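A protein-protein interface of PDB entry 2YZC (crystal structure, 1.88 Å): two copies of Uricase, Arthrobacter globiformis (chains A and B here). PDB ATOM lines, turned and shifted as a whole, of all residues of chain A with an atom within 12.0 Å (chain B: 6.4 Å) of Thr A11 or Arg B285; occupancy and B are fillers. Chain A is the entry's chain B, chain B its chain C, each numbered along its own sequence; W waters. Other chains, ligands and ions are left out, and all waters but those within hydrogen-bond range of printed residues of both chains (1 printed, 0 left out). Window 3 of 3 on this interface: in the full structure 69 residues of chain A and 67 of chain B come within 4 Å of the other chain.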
ATOM      1  N   THR A  11     -25.511  -4.989   5.069  1.00  0.00           N
ATOM      2  CA  THR A  11     -24.842  -4.023   5.989  1.00  0.00           C
ATOM      3  C   THR A  11     -24.922  -4.493   7.437  1.00  0.00           C
ATOM      4  O   THR A  11     -23.903  -4.825   8.039  1.00  0.00           O
ATOM      5  CB  THR A  11     -25.474  -2.646   5.853  1.00  0.00           C
ATOM      6  N   LYS A  12     -26.127  -4.516   7.998  1.00  0.00           N
ATOM      7  CA  LYS A  12     -26.307  -4.956   9.380  1.00  0.00           C
ATOM      8  C   LYS A  12     -26.836  -6.387   9.421  1.00  0.00           C
ATOM      9  O   LYS A  12     -27.793  -6.728   8.724  1.00  0.00           O
ATOM     10  CB  LYS A  12     -27.265  -4.017  10.114  1.00  0.00           C
ATOM     11  N   VAL A  13     -26.206  -7.217  10.249  1.00  0.00           N
ATOM     12  CA  VAL A  13     -26.584  -8.621  10.387  1.00  0.00           C
ATOM     13  C   VAL A  13     -27.159  -8.933  11.767  1.00  0.00           C
ATOM     14  O   VAL A  13     -26.726  -8.372  12.773  1.00  0.00           O
ATOM     15  CB  VAL A  13     -25.363  -9.527  10.133  1.00  0.00           C
ATOM     16  CG1 VAL A  13     -25.628 -10.924  10.651  1.00  0.00           C
ATOM     17  CG2 VAL A  13     -25.054  -9.558   8.650  1.00  0.00           C
ATOM     18  N   VAL A  14     -28.127  -9.842  11.808  1.00  0.00           N
ATOM     19  CA  VAL A  14     -28.769 -10.213  13.063  1.00  0.00           C
ATOM     20  C   VAL A  14     -28.865 -11.721  13.265  1.00  0.00           C
ATOM     21  O   VAL A  14     -29.149 -12.466  12.327  1.00  0.00           O
ATOM     22  CB  VAL A  14     -30.200  -9.631  13.144  1.00  0.00           C
ATOM     23  CG1 VAL A  14     -30.866 -10.059  14.437  1.00  0.00           C
ATOM     24  CG2 VAL A  14     -30.152  -8.114  13.043  1.00  0.00           C
ATOM     25  N   LEU A  15     -28.635 -12.162  14.498  1.00  0.00           N
ATOM     26  CA  LEU A  15     -28.719 -13.576  14.839  1.00  0.00           C
ATOM     27  C   LEU A  15     -30.199 -13.924  14.932  1.00  0.00           C
ATOM     28  O   LEU A  15     -30.936 -13.330  15.721  1.00  0.00           O
ATOM     29  CB  LEU A  15     -28.059 -13.839  16.193  1.00  0.00           C
ATOM     30  CG  LEU A  15     -27.611 -15.260  16.554  1.00  0.00           C
ATOM     31  CD1 LEU A  15     -27.586 -15.382  18.070  1.00  0.00           C
ATOM     32  CD2 LEU A  15     -28.539 -16.305  15.966  1.00  0.00           C
ATOM     33  N   GLY A  16     -30.631 -14.887  14.127  1.00  0.00           N
ATOM     34  CA  GLY A  16     -32.021 -15.293  14.149  1.00  0.00           C
ATOM     35  C   GLY A  16     -32.224 -16.527  15.004  1.00  0.00           C
ATOM     36  O   GLY A  16     -31.569 -16.693  16.037  1.00  0.00           O
ATOM     37  N   GLN A  17     -33.140 -17.391  14.575  1.00  0.00           N
ATOM     38  CA  GLN A  17     -33.430 -18.622  15.295  1.00  0.00           C
ATOM     39  C   GLN A  17     -32.143 -19.446  15.378  1.00  0.00           C
ATOM     40  O   GLN A  17     -31.347 -19.451  14.442  1.00  0.00           O
ATOM     41  CB  GLN A  17     -34.523 -19.409  14.560  1.00  0.00           C
ATOM     42  CG  GLN A  17     -35.835 -18.635  14.413  1.00  0.00           C
ATOM     43  CD  GLN A  17     -36.891 -19.372  13.598  1.00  0.00           C
ATOM     44  OE1 GLN A  17     -36.658 -19.747  12.444  1.00  0.00           O
ATOM     45  NE2 GLN A  17     -38.062 -19.572  14.194  1.00  0.00           N
ATOM     46  N   GLU A  53     -26.822 -15.354  22.332  1.00  0.00           N
ATOM     47  CA  GLU A  53     -26.341 -14.241  21.526  1.00  0.00           C
ATOM     48  C   GLU A  53     -24.822 -14.085  21.601  1.00  0.00           C
ATOM     49  O   GLU A  53     -24.143 -14.069  20.574  1.00  0.00           O
ATOM     50  CB  GLU A  53     -27.019 -12.948  21.993  1.00  0.00           C
ATOM     51  CG  GLU A  53     -26.707 -11.712  21.164  1.00  0.00           C
ATOM     52  CD  GLU A  53     -27.401 -11.714  19.815  1.00  0.00           C
ATOM     53  OE1 GLU A  53     -28.492 -12.316  19.703  1.00  0.00           O
ATOM     54  OE2 GLU A  53     -26.865 -11.097  18.869  1.00  0.00           O
ATOM     55  N   ASN B 193     -33.628 -12.534  -2.342  1.00  0.00           N
ATOM     56  CA  ASN B 193     -34.709 -11.555  -2.240  1.00  0.00           C
ATOM     57  C   ASN B 193     -35.122 -11.015  -3.612  1.00  0.00           C
ATOM     58  O   ASN B 193     -35.858 -10.029  -3.711  1.00  0.00           O
ATOM     59  CB  ASN B 193     -34.293 -10.404  -1.311  1.00  0.00           C
ATOM     60  CG  ASN B 193     -33.004  -9.729  -1.747  1.00  0.00           C
ATOM     61  OD1 ASN B 193     -32.199  -9.303  -0.912  1.00  0.00           O
ATOM     62  ND2 ASN B 193     -32.810  -9.613  -3.049  1.00  0.00           N
ATOM     63  N   VAL B 233     -21.398 -13.811   4.227  1.00  0.00           N
ATOM     64  CA  VAL B 233     -22.286 -13.971   3.083  1.00  0.00           C
ATOM     65  C   VAL B 233     -23.273 -12.808   2.949  1.00  0.00           C
ATOM     66  O   VAL B 233     -23.397 -12.211   1.876  1.00  0.00           O
ATOM     67  CB  VAL B 233     -23.068 -15.300   3.175  1.00  0.00           C
ATOM     68  CG1 VAL B 233     -24.105 -15.383   2.061  1.00  0.00           C
ATOM     69  CG2 VAL B 233     -22.096 -16.476   3.080  1.00  0.00           C
ATOM     70  N   ILE B 234     -23.968 -12.490   4.036  1.00  0.00           N
ATOM     71  CA  ILE B 234     -24.952 -11.410   4.015  1.00  0.00           C
ATOM     72  C   ILE B 234     -24.325 -10.063   3.679  1.00  0.00           C
ATOM     73  O   ILE B 234     -24.880  -9.298   2.894  1.00  0.00           O
ATOM     74  CB  ILE B 234     -25.698 -11.288   5.367  1.00  0.00           C
ATOM     75  CG1 ILE B 234     -26.432 -12.596   5.683  1.00  0.00           C
ATOM     76  CG2 ILE B 234     -26.692 -10.128   5.311  1.00  0.00           C
ATOM     77  CD1 ILE B 234     -27.430 -13.022   4.623  1.00  0.00           C
ATOM     78  N   GLU B 235     -23.166  -9.777   4.267  1.00  0.00           N
ATOM     79  CA  GLU B 235     -22.489  -8.510   4.012  1.00  0.00           C
ATOM     80  C   GLU B 235     -22.002  -8.388   2.572  1.00  0.00           C
ATOM     81  O   GLU B 235     -21.898  -7.286   2.039  1.00  0.00           O
ATOM     82  CB  GLU B 235     -21.302  -8.332   4.972  1.00  0.00           C
ATOM     83  CG  GLU B 235     -21.709  -8.002   6.407  1.00  0.00           C
ATOM     84  CD  GLU B 235     -20.520  -7.885   7.354  1.00  0.00           C
ATOM     85  OE1 GLU B 235     -20.719  -7.445   8.507  1.00  0.00           O
ATOM     86  OE2 GLU B 235     -19.392  -8.239   6.951  1.00  0.00           O
ATOM     87  N   THR B 236     -21.722  -9.519   1.938  1.00  0.00           N
ATOM     88  CA  THR B 236     -21.219  -9.512   0.569  1.00  0.00           C
ATOM     89  C   THR B 236     -22.278  -9.520  -0.529  1.00  0.00           C
ATOM     90  O   THR B 236     -22.078  -8.917  -1.583  1.00  0.00           O
ATOM     91  CB  THR B 236     -20.284 -10.719   0.320  1.00  0.00           C
ATOM     92  OG1 THR B 236     -19.214 -10.701   1.273  1.00  0.00           O
ATOM     93  CG2 THR B 236     -19.701 -10.662  -1.088  1.00  0.00           C
ATOM     94  N   HIS B 237     -23.395 -10.202  -0.298  1.00  0.00           N
ATOM     95  CA  HIS B 237     -24.426 -10.285  -1.324  1.00  0.00           C
ATOM     96  C   HIS B 237     -25.762  -9.641  -0.997  1.00  0.00           C
ATOM     97  O   HIS B 237     -26.536 -10.164  -0.198  1.00  0.00           O
ATOM     98  CB  HIS B 237     -24.661 -11.744  -1.709  1.00  0.00           C
ATOM     99  CG  HIS B 237     -23.489 -12.382  -2.385  1.00  0.00           C
ATOM    100  ND1 HIS B 237     -22.468 -12.990  -1.688  1.00  0.00           N
ATOM    101  CD2 HIS B 237     -23.161 -12.475  -3.694  1.00  0.00           C
ATOM    102  CE1 HIS B 237     -21.561 -13.431  -2.540  1.00  0.00           C
ATOM    103  NE2 HIS B 237     -21.956 -13.132  -3.764  1.00  0.00           N
ATOM    104  N   PRO B 238     -26.056  -8.498  -1.638  1.00  0.00           N
ATOM    105  CA  PRO B 238     -27.305  -7.756  -1.434  1.00  0.00           C
ATOM    106  C   PRO B 238     -28.542  -8.569  -1.813  1.00  0.00           C
ATOM    107  O   PRO B 238     -29.636  -8.299  -1.329  1.00  0.00           O
ATOM    108  CB  PRO B 238     -27.133  -6.531  -2.333  1.00  0.00           C
ATOM    109  CG  PRO B 238     -25.648  -6.359  -2.411  1.00  0.00           C
ATOM    110  CD  PRO B 238     -25.163  -7.773  -2.557  1.00  0.00           C
ATOM    111  N   GLU B 239     -28.369  -9.567  -2.676  1.00  0.00           N
ATOM    112  CA  GLU B 239     -29.499 -10.391  -3.103  1.00  0.00           C
ATOM    113  C   GLU B 239     -29.899 -11.482  -2.112  1.00  0.00           C
ATOM    114  O   GLU B 239     -30.854 -12.216  -2.357  1.00  0.00           O
ATOM    115  CB  GLU B 239     -29.215 -11.032  -4.468  1.00  0.00           C
ATOM    116  CG  GLU B 239     -27.885 -11.743  -4.558  1.00  0.00           C
ATOM    117  CD  GLU B 239     -26.773 -10.825  -5.024  1.00  0.00           C
ATOM    118  OE1 GLU B 239     -26.704 -10.544  -6.239  1.00  0.00           O
ATOM    119  OE2 GLU B 239     -25.976 -10.377  -4.177  1.00  0.00           O
ATOM    120  N   ILE B 240     -29.183 -11.583  -0.996  1.00  0.00           N
ATOM    121  CA  ILE B 240     -29.480 -12.594   0.020  1.00  0.00           C
ATOM    122  C   ILE B 240     -30.027 -11.966   1.302  1.00  0.00           C
ATOM    123  O   ILE B 240     -29.410 -11.069   1.870  1.00  0.00           O
ATOM    124  CB  ILE B 240     -28.210 -13.409   0.385  1.00  0.00           C
ATOM    125  CG1 ILE B 240     -27.664 -14.123  -0.855  1.00  0.00           C
ATOM    126  CG2 ILE B 240     -28.542 -14.417   1.477  1.00  0.00           C
ATOM    127  CD1 ILE B 240     -26.331 -14.842  -0.624  1.00  0.00           C
ATOM    128  N   ASP B 241     -31.183 -12.437   1.761  1.00  0.00           N
ATOM    129  CA  ASP B 241     -31.771 -11.897   2.980  1.00  0.00           C
ATOM    130  C   ASP B 241     -31.436 -12.697   4.233  1.00  0.00           C
ATOM    131  O   ASP B 241     -31.467 -12.158   5.336  1.00  0.00           O
ATOM    132  CB  ASP B 241     -33.292 -11.773   2.840  1.00  0.00           C
ATOM    133  CG  ASP B 241     -33.719 -10.433   2.245  1.00  0.00           C
ATOM    134  OD1 ASP B 241     -32.842  -9.602   1.923  1.00  0.00           O
ATOM    135  OD2 ASP B 241     -34.939 -10.212   2.105  1.00  0.00           O
ATOM    136  N   GLU B 242     -31.117 -13.979   4.075  1.00  0.00           N
ATOM    137  CA  GLU B 242     -30.775 -14.805   5.228  1.00  0.00           C
ATOM    138  C   GLU B 242     -30.092 -16.089   4.799  1.00  0.00           C
ATOM    139  O   GLU B 242     -30.231 -16.533   3.664  1.00  0.00           O
ATOM    140  CB  GLU B 242     -32.025 -15.157   6.040  1.00  0.00           C
ATOM    141  CG  GLU B 242     -33.125 -15.810   5.227  1.00  0.00           C
ATOM    142  CD  GLU B 242     -34.342 -16.180   6.058  1.00  0.00           C
ATOM    143  OE1 GLU B 242     -35.424 -16.354   5.461  1.00  0.00           O
ATOM    144  OE2 GLU B 242     -34.217 -16.307   7.299  1.00  0.00           O
ATOM    145  N   ILE B 283     -28.678 -16.572  10.173  1.00  0.00           N
ATOM    146  CA  ILE B 283     -28.070 -15.246  10.196  1.00  0.00           C
ATOM    147  C   ILE B 283     -28.894 -14.449   9.187  1.00  0.00           C
ATOM    148  O   ILE B 283     -28.990 -14.832   8.020  1.00  0.00           O
ATOM    149  CB  ILE B 283     -26.585 -15.286   9.771  1.00  0.00           C
ATOM    150  CG1 ILE B 283     -25.744 -15.991  10.842  1.00  0.00           C
ATOM    151  CG2 ILE B 283     -26.051 -13.882   9.599  1.00  0.00           C
ATOM    152  CD1 ILE B 283     -26.052 -17.460  11.009  1.00  0.00           C
ATOM    153  N   GLN B 284     -29.490 -13.348   9.637  1.00  0.00           N
ATOM    154  CA  GLN B 284     -30.350 -12.543   8.771  1.00  0.00           C
ATOM    155  C   GLN B 284     -29.949 -11.083   8.570  1.00  0.00           C
ATOM    156  O   GLN B 284     -29.305 -10.471   9.420  1.00  0.00           O
ATOM    157  CB  GLN B 284     -31.784 -12.559   9.317  1.00  0.00           C
ATOM    158  CG  GLN B 284     -32.449 -13.926   9.365  1.00  0.00           C
ATOM    159  CD  GLN B 284     -33.864 -13.875   9.929  1.00  0.00           C
ATOM    160  OE1 GLN B 284     -34.710 -14.706   9.588  1.00  0.00           O
ATOM    161  NE2 GLN B 284     -34.123 -12.907  10.804  1.00  0.00           N
ATOM    162  N   ARG B 285     -30.347 -10.537   7.424  1.00  0.00           N
ATOM    163  CA  ARG B 285     -30.119  -9.134   7.113  1.00  0.00           C
ATOM    164  C   ARG B 285     -31.102  -8.462   8.068  1.00  0.00           C
ATOM    165  O   ARG B 285     -32.264  -8.868   8.144  1.00  0.00           O
ATOM    166  CB  ARG B 285     -30.517  -8.863   5.657  1.00  0.00           C
ATOM    167  CG  ARG B 285     -30.471  -7.413   5.207  1.00  0.00           C
ATOM    168  CD  ARG B 285     -30.845  -7.338   3.730  1.00  0.00           C
ATOM    169  NE  ARG B 285     -29.954  -8.178   2.936  1.00  0.00           N
ATOM    170  CZ  ARG B 285     -28.730  -7.824   2.560  1.00  0.00           C
ATOM    171  NH1 ARG B 285     -28.253  -6.632   2.893  1.00  0.00           N
ATOM    172  NH2 ARG B 285     -27.969  -8.671   1.879  1.00  0.00           N
ATOM    173  N   GLU B 286     -30.644  -7.458   8.810  1.00  0.00           N
ATOM    174  CA  GLU B 286     -31.514  -6.787   9.772  1.00  0.00           C
ATOM    175  C   GLU B 286     -32.827  -6.305   9.167  1.00  0.00           C
ATOM    176  O   GLU B 286     -32.833  -5.649   8.132  1.00  0.00           O
ATOM    177  CB  GLU B 286     -30.799  -5.594  10.408  1.00  0.00           C
ATOM    178  CG  GLU B 286     -31.626  -4.930  11.503  1.00  0.00           C
ATOM    179  CD  GLU B 286     -31.019  -3.639  12.012  1.00  0.00           C
ATOM    180  OE1 GLU B 286     -31.581  -3.066  12.970  1.00  0.00           O
ATOM    181  OE2 GLU B 286     -29.991  -3.191  11.457  1.00  0.00           O
ATOM    182  N   GLY B 287     -33.937  -6.651   9.812  1.00  0.00           N
ATOM    183  CA  GLY B 287     -35.236  -6.211   9.332  1.00  0.00           C
ATOM    184  C   GLY B 287     -35.925  -7.060   8.283  1.00  0.00           C
ATOM    185  O   GLY B 287     -37.061  -6.767   7.902  1.00  0.00           O
ATOM    186  N   SER B 288     -35.264  -8.111   7.808  1.00  0.00           N
ATOM    187  CA  SER B 288     -35.872  -8.968   6.795  1.00  0.00           C
ATOM    188  C   SER B 288     -36.927  -9.880   7.419  1.00  0.00           C
ATOM    189  O   SER B 288     -37.060  -9.943   8.642  1.00  0.00           O
ATOM    190  CB  SER B 288     -34.796  -9.798   6.092  1.00  0.00           C
ATOM    191  OG  SER B 288     -34.029 -10.527   7.026  1.00  0.00           O
ATOM    192  N   ARG B 289     -37.676 -10.582   6.575  1.00  0.00           N
ATOM    193  CA  ARG B 289     -38.731 -11.470   7.048  1.00  0.00           C
ATOM    194  C   ARG B 289     -38.216 -12.462   8.089  1.00  0.00           C
ATOM    195  O   ARG B 289     -37.176 -13.095   7.899  1.00  0.00           O
ATOM    196  CB  ARG B 289     -39.352 -12.213   5.868  1.00  0.00           C
ATOM    197  CG  ARG B 289     -40.676 -12.873   6.199  1.00  0.00           C
ATOM    198  CD  ARG B 289     -41.456 -13.140   4.939  1.00  0.00           C
ATOM    199  NE  ARG B 289     -42.772 -13.707   5.205  1.00  0.00           N
ATOM    200  CZ  ARG B 289     -43.646 -14.010   4.253  1.00  0.00           C
ATOM    201  NH1 ARG B 289     -43.334 -13.793   2.983  1.00  0.00           N
ATOM    202  NH2 ARG B 289     -44.823 -14.534   4.567  1.00  0.00           N
HETATM  203  O   HOH W   1     -34.633 -16.652  12.196  1.00  0.00           O
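O of Lys A12 sits at hydrogen-bond distance from N of Glu B286 (2.9 Å). The backbone NH (N) of Val A14 sits at hydrogen-bond distance from the backbone carbonyl oxygen (O) of Gln B284.
The backbone carbonyl oxygen (O) of Ile B234 is in hydrogen-bond range of the guanidinium group (NH2) of Arg B285 (3.3 Å). The backbone carbonyl oxygen of His B237 is in hydrogen-bond range of the guanidinium group of Arg B285 (2.9 Å). NH2 of Arg B285 lies within hydrogen-bond range of O of Ile B240, 2.8 Å away. OE2 of Glu B242 lies close to OE1 of Gln B284, at 2.8 Å. O of Arg B289 lies close to OE1 of Gln B284, 3.4 Å away. OG of Ser B288 is in hydrogen-bond range of O of Arg B285, at 2.7 Å.
Among the printed residues, merely in contact across the chains: Thr A11 with Arg B285, Lys A12 with Arg B285, Val A13 with Ile B234, Val A13 with Ile B283, Val A13 with Gln B284, Val A14 with Ile B283 and Val A14 with Glu B286.
Thr A11 touches just one residue of chain B: Arg B285 (3.9 Å). No residue of chain A comes within 4 Å of Glu B235. No residue of chain A comes within 4 Å of Pro B238. No residue of chain A comes within 4 Å of Asp B241. Printed residues of chain A within 4 Å of Gln B284: Val A13 (3.4 Å) and Val A14 (2.7 Å). Printed residues of chain A within 4 Å of Ile B283: Val A13 (3.2 Å) and Val A14 (3.7 Å). Of the printed residues of chain B, Val A13 touches Ile B234 (3.8 Å), Ile B283 (3.2 Å) and Gln B284 (3.4 Å). Of the printed residues of chain B, Lys A12 touches Arg B285 (3.7 Å) and Glu B286 (2.9 Å). Of the printed residues of chain B, Val A14 touches Ile B283, Gln B284 and Glu B286. Gln A17 touches none of the printed residues of chain B. The nearest residue of chain A that does not touch Arg B285 is Val A13 (4.8 Å).
Of the 8 printed residues of chain A, 4 touch a printed residue of chain B. Hydrophobic or aromatic side chains of chain A that line the printed part of chain B: Val A13 and Val A14. Along chain A the printed residues that touch a printed residue of chain B span positions 11 to 14. Hydrophobic or aromatic side chains of chain B that line the printed part of chain A: Ile B234 and Ile B283. Along chain B the printed residues that touch a printed residue of chain A span positions 234 to 286. Among the printed residues, no Asp or Glu carboxylate lies within 4 Å of a Lys or Arg side-chain nitrogen of the other chain.
No position is printed for both chains.
Water W1 bridges the backbone NH (N) of Gln A17 (2.9 Å) and the side-chain amide oxygen (OE1) of Gln B284 (3.3 Å).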
